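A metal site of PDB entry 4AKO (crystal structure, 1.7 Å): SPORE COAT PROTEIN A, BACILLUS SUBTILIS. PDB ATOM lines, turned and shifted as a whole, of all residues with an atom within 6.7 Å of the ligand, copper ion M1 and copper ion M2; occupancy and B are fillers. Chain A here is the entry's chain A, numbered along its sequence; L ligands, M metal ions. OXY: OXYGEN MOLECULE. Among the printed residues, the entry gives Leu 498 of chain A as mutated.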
ATOM      1  N   HIS A 105      -4.000 -17.597  -1.968  1.00  0.00           N
ATOM      2  CA  HIS A 105      -4.068 -18.308  -0.704  1.00  0.00           C
ATOM      3  C   HIS A 105      -5.290 -17.849   0.087  1.00  0.00           C
ATOM      4  O   HIS A 105      -5.477 -16.654   0.309  1.00  0.00           O
ATOM      5  CB  HIS A 105      -2.805 -18.064   0.100  1.00  0.00           C
ATOM      6  CG  HIS A 105      -2.890 -18.595   1.495  1.00  0.00           C
ATOM      7  ND1 HIS A 105      -3.202 -19.917   1.750  1.00  0.00           N
ATOM      8  CD2 HIS A 105      -2.737 -18.008   2.696  1.00  0.00           C
ATOM      9  CE1 HIS A 105      -3.227 -20.120   3.058  1.00  0.00           C
ATOM     10  NE2 HIS A 105      -2.946 -18.969   3.649  1.00  0.00           N
ATOM     11  N   LEU A 106      -6.125 -18.802   0.490  1.00  0.00           N
ATOM     12  CA  LEU A 106      -7.220 -18.525   1.416  1.00  0.00           C
ATOM     13  C   LEU A 106      -6.678 -18.654   2.837  1.00  0.00           C
ATOM     14  O   LEU A 106      -6.510 -19.768   3.360  1.00  0.00           O
ATOM     15  CB  LEU A 106      -8.409 -19.461   1.175  1.00  0.00           C
ATOM     16  CG  LEU A 106      -9.578 -19.321   2.175  1.00  0.00           C
ATOM     17  CD1 LEU A 106     -10.130 -17.897   2.137  1.00  0.00           C
ATOM     18  CD2 LEU A 106     -10.679 -20.334   1.887  1.00  0.00           C
ATOM     19  N   HIS A 107      -6.373 -17.492   3.419  1.00  0.00           N
ATOM     20  CA  HIS A 107      -5.745 -17.418   4.724  1.00  0.00           C
ATOM     21  C   HIS A 107      -6.704 -17.888   5.823  1.00  0.00           C
ATOM     22  O   HIS A 107      -7.758 -17.299   6.040  1.00  0.00           O
ATOM     23  CB  HIS A 107      -5.277 -15.986   4.987  1.00  0.00           C
ATOM     24  CG  HIS A 107      -4.443 -15.833   6.215  1.00  0.00           C
ATOM     25  ND1 HIS A 107      -3.142 -15.376   6.174  1.00  0.00           N
ATOM     26  CD2 HIS A 107      -4.715 -16.085   7.513  1.00  0.00           C
ATOM     27  CE1 HIS A 107      -2.646 -15.362   7.398  1.00  0.00           C
ATOM     28  NE2 HIS A 107      -3.581 -15.777   8.234  1.00  0.00           N
ATOM     29  N   GLY A 108      -6.302 -18.960   6.519  1.00  0.00           N
ATOM     30  CA  GLY A 108      -7.133 -19.604   7.522  1.00  0.00           C
ATOM     31  C   GLY A 108      -7.917 -20.811   6.995  1.00  0.00           C
ATOM     32  O   GLY A 108      -8.608 -21.497   7.751  1.00  0.00           O
ATOM     33  N   ASP A 116      -4.244 -24.722  -1.590  1.00  0.00           N
ATOM     34  CA  ASP A 116      -3.866 -23.813  -0.502  1.00  0.00           C
ATOM     35  C   ASP A 116      -3.120 -22.555  -0.976  1.00  0.00           C
ATOM     36  O   ASP A 116      -2.965 -21.601  -0.218  1.00  0.00           O
ATOM     37  CB  ASP A 116      -3.045 -24.560   0.556  1.00  0.00           C
ATOM     38  CG  ASP A 116      -2.868 -23.754   1.831  1.00  0.00           C
ATOM     39  OD1 ASP A 116      -3.873 -23.214   2.331  1.00  0.00           O
ATOM     40  OD2 ASP A 116      -1.719 -23.658   2.299  1.00  0.00           O
ATOM     41  N   GLY A 117      -2.678 -22.557  -2.231  1.00  0.00           N
ATOM     42  CA  GLY A 117      -1.938 -21.427  -2.776  1.00  0.00           C
ATOM     43  C   GLY A 117      -0.460 -21.474  -2.424  1.00  0.00           C
ATOM     44  O   GLY A 117       0.117 -20.479  -1.983  1.00  0.00           O
ATOM     45  N   PRO A 119       3.408 -21.192  -2.631  1.00  0.00           N
ATOM     46  CA  PRO A 119       4.145 -20.116  -3.320  1.00  0.00           C
ATOM     47  C   PRO A 119       4.667 -20.525  -4.698  1.00  0.00           C
ATOM     48  O   PRO A 119       4.758 -19.679  -5.578  1.00  0.00           O
ATOM     49  CB  PRO A 119       5.315 -19.824  -2.368  1.00  0.00           C
ATOM     50  CG  PRO A 119       4.805 -20.237  -1.019  1.00  0.00           C
ATOM     51  CD  PRO A 119       3.975 -21.453  -1.289  1.00  0.00           C
ATOM     52  N   TRP A 151      -9.508 -14.553   4.979  1.00  0.00           N
ATOM     53  CA  TRP A 151      -9.295 -13.596   3.912  1.00  0.00           C
ATOM     54  C   TRP A 151      -8.418 -14.224   2.863  1.00  0.00           C
ATOM     55  O   TRP A 151      -7.734 -15.204   3.136  1.00  0.00           O
ATOM     56  CB  TRP A 151      -8.722 -12.265   4.440  1.00  0.00           C
ATOM     57  CG  TRP A 151      -7.343 -12.279   5.011  1.00  0.00           C
ATOM     58  CD1 TRP A 151      -6.906 -12.962   6.125  1.00  0.00           C
ATOM     59  CD2 TRP A 151      -6.230 -11.514   4.542  1.00  0.00           C
ATOM     60  NE1 TRP A 151      -5.575 -12.681   6.352  1.00  0.00           N
ATOM     61  CE2 TRP A 151      -5.143 -11.794   5.399  1.00  0.00           C
ATOM     62  CE3 TRP A 151      -6.044 -10.622   3.478  1.00  0.00           C
ATOM     63  CZ2 TRP A 151      -3.874 -11.206   5.221  1.00  0.00           C
ATOM     64  CZ3 TRP A 151      -4.792 -10.036   3.296  1.00  0.00           C
ATOM     65  CH2 TRP A 151      -3.722 -10.342   4.165  1.00  0.00           C
ATOM     66  N   HIS A 153      -5.639 -13.687  -0.505  1.00  0.00           N
ATOM     67  CA  HIS A 153      -4.639 -12.765  -1.041  1.00  0.00           C
ATOM     68  C   HIS A 153      -3.611 -13.515  -1.872  1.00  0.00           C
ATOM     69  O   HIS A 153      -3.512 -14.747  -1.786  1.00  0.00           O
ATOM     70  CB  HIS A 153      -3.948 -11.970   0.086  1.00  0.00           C
ATOM     71  CG  HIS A 153      -3.194 -12.823   1.069  1.00  0.00           C
ATOM     72  ND1 HIS A 153      -1.926 -13.307   0.804  1.00  0.00           N
ATOM     73  CD2 HIS A 153      -3.513 -13.238   2.317  1.00  0.00           C
ATOM     74  CE1 HIS A 153      -1.505 -13.998   1.851  1.00  0.00           C
ATOM     75  NE2 HIS A 153      -2.446 -13.975   2.781  1.00  0.00           N
ATOM     76  N   ASP A 154      -2.859 -12.779  -2.669  1.00  0.00           N
ATOM     77  CA  ASP A 154      -1.811 -13.394  -3.470  1.00  0.00           C
ATOM     78  C   ASP A 154      -0.694 -13.975  -2.616  1.00  0.00           C
ATOM     79  O   ASP A 154      -0.381 -13.427  -1.550  1.00  0.00           O
ATOM     80  CB  ASP A 154      -1.218 -12.407  -4.465  1.00  0.00           C
ATOM     81  CG  ASP A 154      -0.346 -13.092  -5.485  1.00  0.00           C
ATOM     82  OD1 ASP A 154      -0.902 -13.727  -6.395  1.00  0.00           O
ATOM     83  OD2 ASP A 154       0.903 -13.033  -5.336  1.00  0.00           O
ATOM     84  N   HIS A 155      -0.073 -15.051  -3.081  1.00  0.00           N
ATOM     85  CA  HIS A 155       0.999 -15.711  -2.343  1.00  0.00           C
ATOM     86  C   HIS A 155       2.150 -16.145  -3.242  1.00  0.00           C
ATOM     87  O   HIS A 155       2.902 -17.054  -2.907  1.00  0.00           O
ATOM     88  CB  HIS A 155       0.438 -16.932  -1.583  1.00  0.00           C
ATOM     89  CG  HIS A 155       1.090 -17.192  -0.254  1.00  0.00           C
ATOM     90  ND1 HIS A 155       2.456 -17.367  -0.108  1.00  0.00           N
ATOM     91  CD2 HIS A 155       0.567 -17.339   0.988  1.00  0.00           C
ATOM     92  CE1 HIS A 155       2.735 -17.581   1.164  1.00  0.00           C
ATOM     93  NE2 HIS A 155       1.606 -17.583   1.850  1.00  0.00           N
ATOM     94  N   THR A 160       4.956 -11.646  -3.184  1.00  0.00           N
ATOM     95  CA  THR A 160       3.801 -11.468  -2.312  1.00  0.00           C
ATOM     96  C   THR A 160       3.652 -10.020  -1.828  1.00  0.00           C
ATOM     97  O   THR A 160       2.547  -9.474  -1.843  1.00  0.00           O
ATOM     98  CB  THR A 160       3.825 -12.514  -1.162  1.00  0.00           C
ATOM     99  OG1 THR A 160       3.791 -13.833  -1.733  1.00  0.00           O
ATOM    100  CG2 THR A 160       2.637 -12.346  -0.238  1.00  0.00           C
ATOM    101  N   ALA A 297      -2.256  -9.786   9.012  1.00  0.00           N
ATOM    102  CA  ALA A 297      -3.008 -11.054   8.859  1.00  0.00           C
ATOM    103  C   ALA A 297      -3.843 -11.485  10.060  1.00  0.00           C
ATOM    104  O   ALA A 297      -4.592 -12.463   9.961  1.00  0.00           O
ATOM    105  CB  ALA A 297      -2.116 -12.194   8.382  1.00  0.00           C
ATOM    106  N   HIS A 422       2.688 -17.094  10.994  1.00  0.00           N
ATOM    107  CA  HIS A 422       1.528 -17.757  10.453  1.00  0.00           C
ATOM    108  C   HIS A 422       1.829 -19.189  10.033  1.00  0.00           C
ATOM    109  O   HIS A 422       2.806 -19.446   9.344  1.00  0.00           O
ATOM    110  CB  HIS A 422       0.994 -16.969   9.254  1.00  0.00           C
ATOM    111  CG  HIS A 422      -0.170 -17.620   8.596  1.00  0.00           C
ATOM    112  ND1 HIS A 422      -1.277 -18.022   9.306  1.00  0.00           N
ATOM    113  CD2 HIS A 422      -0.415 -17.945   7.309  1.00  0.00           C
ATOM    114  CE1 HIS A 422      -2.145 -18.579   8.488  1.00  0.00           C
ATOM    115  NE2 HIS A 422      -1.642 -18.548   7.273  1.00  0.00           N
ATOM    116  N   LEU A 423       0.983 -20.129  10.484  1.00  0.00           N
ATOM    117  CA  LEU A 423       1.034 -21.514  10.009  1.00  0.00           C
ATOM    118  C   LEU A 423      -0.167 -21.759   9.094  1.00  0.00           C
ATOM    119  O   LEU A 423      -1.298 -21.436   9.459  1.00  0.00           O
ATOM    120  CB  LEU A 423       0.977 -22.507  11.178  1.00  0.00           C
ATOM    121  CG  LEU A 423       2.272 -22.820  11.924  1.00  0.00           C
ATOM    122  CD1 LEU A 423       2.851 -21.574  12.599  1.00  0.00           C
ATOM    123  CD2 LEU A 423       2.039 -23.912  12.961  1.00  0.00           C
ATOM    124  N   HIS A 424       0.080 -22.324   7.925  1.00  0.00           N
ATOM    125  CA  HIS A 424      -1.012 -22.720   7.033  1.00  0.00           C
ATOM    126  C   HIS A 424      -1.755 -23.929   7.586  1.00  0.00           C
ATOM    127  O   HIS A 424      -1.272 -24.597   8.507  1.00  0.00           O
ATOM    128  CB  HIS A 424      -0.473 -23.000   5.635  1.00  0.00           C
ATOM    129  CG  HIS A 424      -0.173 -21.760   4.839  1.00  0.00           C
ATOM    130  ND1 HIS A 424      -0.468 -21.645   3.501  1.00  0.00           N
ATOM    131  CD2 HIS A 424       0.383 -20.577   5.209  1.00  0.00           C
ATOM    132  CE1 HIS A 424      -0.095 -20.454   3.072  1.00  0.00           C
ATOM    133  NE2 HIS A 424       0.425 -19.786   4.090  1.00  0.00           N
ATOM    134  N   THR A 466      -2.306 -16.670  13.152  1.00  0.00           N
ATOM    135  CA  THR A 466      -1.234 -15.706  12.996  1.00  0.00           C
ATOM    136  C   THR A 466      -0.992 -15.090  14.364  1.00  0.00           C
ATOM    137  O   THR A 466      -1.922 -14.554  14.966  1.00  0.00           O
ATOM    138  CB  THR A 466      -1.601 -14.613  11.968  1.00  0.00           C
ATOM    139  OG1 THR A 466      -2.012 -15.242  10.755  1.00  0.00           O
ATOM    140  CG2 THR A 466      -0.406 -13.704  11.692  1.00  0.00           C
ATOM    141  N   VAL A 489       3.067 -24.464   4.246  1.00  0.00           N
ATOM    142  CA  VAL A 489       4.136 -23.530   4.593  1.00  0.00           C
ATOM    143  C   VAL A 489       3.885 -22.926   5.977  1.00  0.00           C
ATOM    144  O   VAL A 489       2.758 -22.959   6.491  1.00  0.00           O
ATOM    145  CB  VAL A 489       4.295 -22.374   3.528  1.00  0.00           C
ATOM    146  CG1 VAL A 489       4.589 -22.921   2.130  1.00  0.00           C
ATOM    147  CG2 VAL A 489       3.100 -21.460   3.504  1.00  0.00           C
ATOM    148  N   TRP A 490       4.930 -22.377   6.577  1.00  0.00           N
ATOM    149  CA  TRP A 490       4.798 -21.495   7.720  1.00  0.00           C
ATOM    150  C   TRP A 490       5.777 -20.341   7.522  1.00  0.00           C
ATOM    151  O   TRP A 490       6.820 -20.503   6.894  1.00  0.00           O
ATOM    152  CB  TRP A 490       5.011 -22.237   9.052  1.00  0.00           C
ATOM    153  CG  TRP A 490       6.435 -22.626   9.349  1.00  0.00           C
ATOM    154  CD1 TRP A 490       7.155 -23.633   8.780  1.00  0.00           C
ATOM    155  CD2 TRP A 490       7.289 -22.020  10.330  1.00  0.00           C
ATOM    156  NE1 TRP A 490       8.424 -23.688   9.337  1.00  0.00           N
ATOM    157  CE2 TRP A 490       8.523 -22.710  10.285  1.00  0.00           C
ATOM    158  CE3 TRP A 490       7.142 -20.963  11.244  1.00  0.00           C
ATOM    159  CZ2 TRP A 490       9.605 -22.382  11.119  1.00  0.00           C
ATOM    160  CZ3 TRP A 490       8.212 -20.629  12.075  1.00  0.00           C
ATOM    161  CH2 TRP A 490       9.430 -21.331  11.999  1.00  0.00           C
ATOM    162  N   HIS A 491       5.431 -19.166   8.037  1.00  0.00           N
ATOM    163  CA  HIS A 491       6.212 -17.965   7.729  1.00  0.00           C
ATOM    164  C   HIS A 491       5.819 -16.771   8.574  1.00  0.00           C
ATOM    165  O   HIS A 491       4.797 -16.761   9.251  1.00  0.00           O
ATOM    166  CB  HIS A 491       6.043 -17.597   6.246  1.00  0.00           C
ATOM    167  CG  HIS A 491       4.625 -17.327   5.837  1.00  0.00           C
ATOM    168  ND1 HIS A 491       4.044 -16.079   5.918  1.00  0.00           N
ATOM    169  CD2 HIS A 491       3.673 -18.150   5.330  1.00  0.00           C
ATOM    170  CE1 HIS A 491       2.799 -16.139   5.496  1.00  0.00           C
ATOM    171  NE2 HIS A 491       2.548 -17.382   5.120  1.00  0.00           N
ATOM    172  N   CYS A 492       6.662 -15.750   8.525  1.00  0.00           N
ATOM    173  CA  CYS A 492       6.306 -14.444   9.036  1.00  0.00           C
ATOM    174  C   CYS A 492       5.376 -13.769   8.038  1.00  0.00           C
ATOM    175  O   CYS A 492       5.594 -13.882   6.821  1.00  0.00           O
ATOM    176  CB  CYS A 492       7.564 -13.610   9.234  1.00  0.00           C
ATOM    177  SG  CYS A 492       7.188 -11.965   9.759  1.00  0.00           S
ATOM    178  N   HIS A 493       4.337 -13.086   8.529  1.00  0.00           N
ATOM    179  CA  HIS A 493       3.378 -12.405   7.647  1.00  0.00           C
ATOM    180  C   HIS A 493       3.680 -10.910   7.432  1.00  0.00           C
ATOM    181  O   HIS A 493       2.856 -10.161   6.891  1.00  0.00           O
ATOM    182  CB  HIS A 493       1.910 -12.649   8.093  1.00  0.00           C
ATOM    183  CG  HIS A 493       0.930 -12.811   6.959  1.00  0.00           C
ATOM    184  ND1 HIS A 493       0.534 -11.767   6.150  1.00  0.00           N
ATOM    185  CD2 HIS A 493       0.225 -13.898   6.532  1.00  0.00           C
ATOM    186  CE1 HIS A 493      -0.341 -12.200   5.263  1.00  0.00           C
ATOM    187  NE2 HIS A 493      -0.554 -13.492   5.471  1.00  0.00           N
ATOM    188  N   LEU A 495       5.222  -9.026   4.926  1.00  0.00           N
ATOM    189  CA  LEU A 495       5.436  -9.522   3.570  1.00  0.00           C
ATOM    190  C   LEU A 495       6.844  -9.252   3.048  1.00  0.00           C
ATOM    191  O   LEU A 495       7.392 -10.046   2.285  1.00  0.00           O
ATOM    192  CB  LEU A 495       4.367  -8.981   2.611  1.00  0.00           C
ATOM    193  CG  LEU A 495       2.928  -9.338   3.006  1.00  0.00           C
ATOM    194  CD1 LEU A 495       1.963  -8.842   1.931  1.00  0.00           C
ATOM    195  CD2 LEU A 495       2.738 -10.849   3.236  1.00  0.00           C
ATOM    196  N   LEU A 498       8.707 -12.177   4.572  1.00  0.00           N
ATOM    197  CA  LEU A 498       8.288 -13.382   3.869  1.00  0.00           C
ATOM    198  C   LEU A 498       9.072 -13.585   2.567  1.00  0.00           C
ATOM    199  O   LEU A 498       9.614 -14.662   2.332  1.00  0.00           O
ATOM    200  CB  LEU A 498       6.770 -13.320   3.595  1.00  0.00           C
ATOM    201  CG  LEU A 498       5.991 -14.530   3.076  1.00  0.00           C
ATOM    202  CD1 LEU A 498       4.512 -14.203   3.180  1.00  0.00           C
ATOM    203  CD2 LEU A 498       6.345 -14.890   1.644  1.00  0.00           C
ATOM    204  N   MET A 503      10.276 -17.747   5.221  1.00  0.00           N
ATOM    205  CA  MET A 503       9.230 -18.699   4.950  1.00  0.00           C
ATOM    206  C   MET A 503       9.840 -20.076   4.739  1.00  0.00           C
ATOM    207  O   MET A 503      10.878 -20.210   4.089  1.00  0.00           O
ATOM    208  CB  MET A 503       8.456 -18.278   3.696  1.00  0.00           C
ATOM    209  CG  MET A 503       7.386 -19.263   3.292  1.00  0.00           C
ATOM    210  SD  MET A 503       6.279 -18.684   2.002  1.00  0.00           S
ATOM    211  CE  MET A 503       7.408 -18.530   0.615  1.00  0.00           C
HETATM  212  O1  OXY L   1      -0.596 -16.492   4.268  1.00  0.00           O
HETATM  213  O2  OXY L   1       0.118 -15.825   3.847  1.00  0.00           O
HETATM  214 CU    CU M   1       1.196 -17.964   3.779  1.00  0.00          CU
HETATM  215 CU    CU M   2      -2.102 -14.562   4.675  1.00  0.00          CU
HETATM  216 CU    CU M   3      -2.165 -18.618   5.404  1.00  0.00          CU
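The backbone NH (N) of His 422 sits at hydrogen-bond distance from the backbone carbonyl oxygen (O) of His 491.
A ring nitrogen (ND1) of His 422 lies close to a ring nitrogen (NE2) of His 107.
The backbone carbonyl oxygen (O) of Trp 151 lies within hydrogen-bond range of the backbone NH (N) of His 107, 2.7 Å away.
OG1 of Thr 466 lies within hydrogen-bond range of NE2 of His 107, at 3.0 Å.
N of His 424 is in hydrogen-bond range of O of Val 489 (3.1 Å).
ND1 of His 424 is in hydrogen-bond range of OD2 of Asp 116, 2.7 Å away.
The backbone carbonyl oxygen of Asp 116 lies within hydrogen-bond range of a ring nitrogen (ND1) of His 105 (2.6 Å).
OG1 of Thr 466 is in hydrogen-bond range of ND1 of His 422 (3.2 Å).
O1 of the ligand lies close to NE2 of His 105, at 3.5 Å.
Merely in contact with the ligand: His 422 (3.4 Å).
Hydrophobic or aromatic side chains within 4 Å of the ligand: His 105, His 107, His 153, His 155, His 422, His 491 and His 493.
Eight residues have an atom within 4 Å of the ligand: His 105, His 107, His 153, His 155, His 422, His 424, His 491 and His 493.
The nearest printed residue that does not touch the ligand is Leu 498 (4.7 Å).
Residues that only touch copper ion M1: His 422 and Val 489.
Along chain A the residues within 4 Å of copper ion M1 span positions 155 to 491.
Trp 151 touches copper ion M2 (CZ2 to CU, 3.8 Å).
Of the 25 residues printed, 4 come within 4 Å of copper ion M2.
Along chain A the residues within 4 Å of copper ion M2 span positions 107 to 493.
The nearest printed residue that does not touch copper ion M2 is His 105 (4.02 Å).
NE2 of His 491 is bound to copper ion M1 (2.0 Å).
Copper ion M1 is bound by NE2 of His 424, 2.0 Å away.
NE2 of His 155 binds copper ion M1 (2.0 Å).
O1 of the ligand binds copper ion M1.
Copper ion M2 is bound by ND1 of His 107 (2.0 Å).
NE2 of His 153 is bound to copper ion M2 (2.0 Å).
NE2 of His 493 binds copper ion M2 (2.0 Å).
Copper ion M2 is bound by O1 of the ligand.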
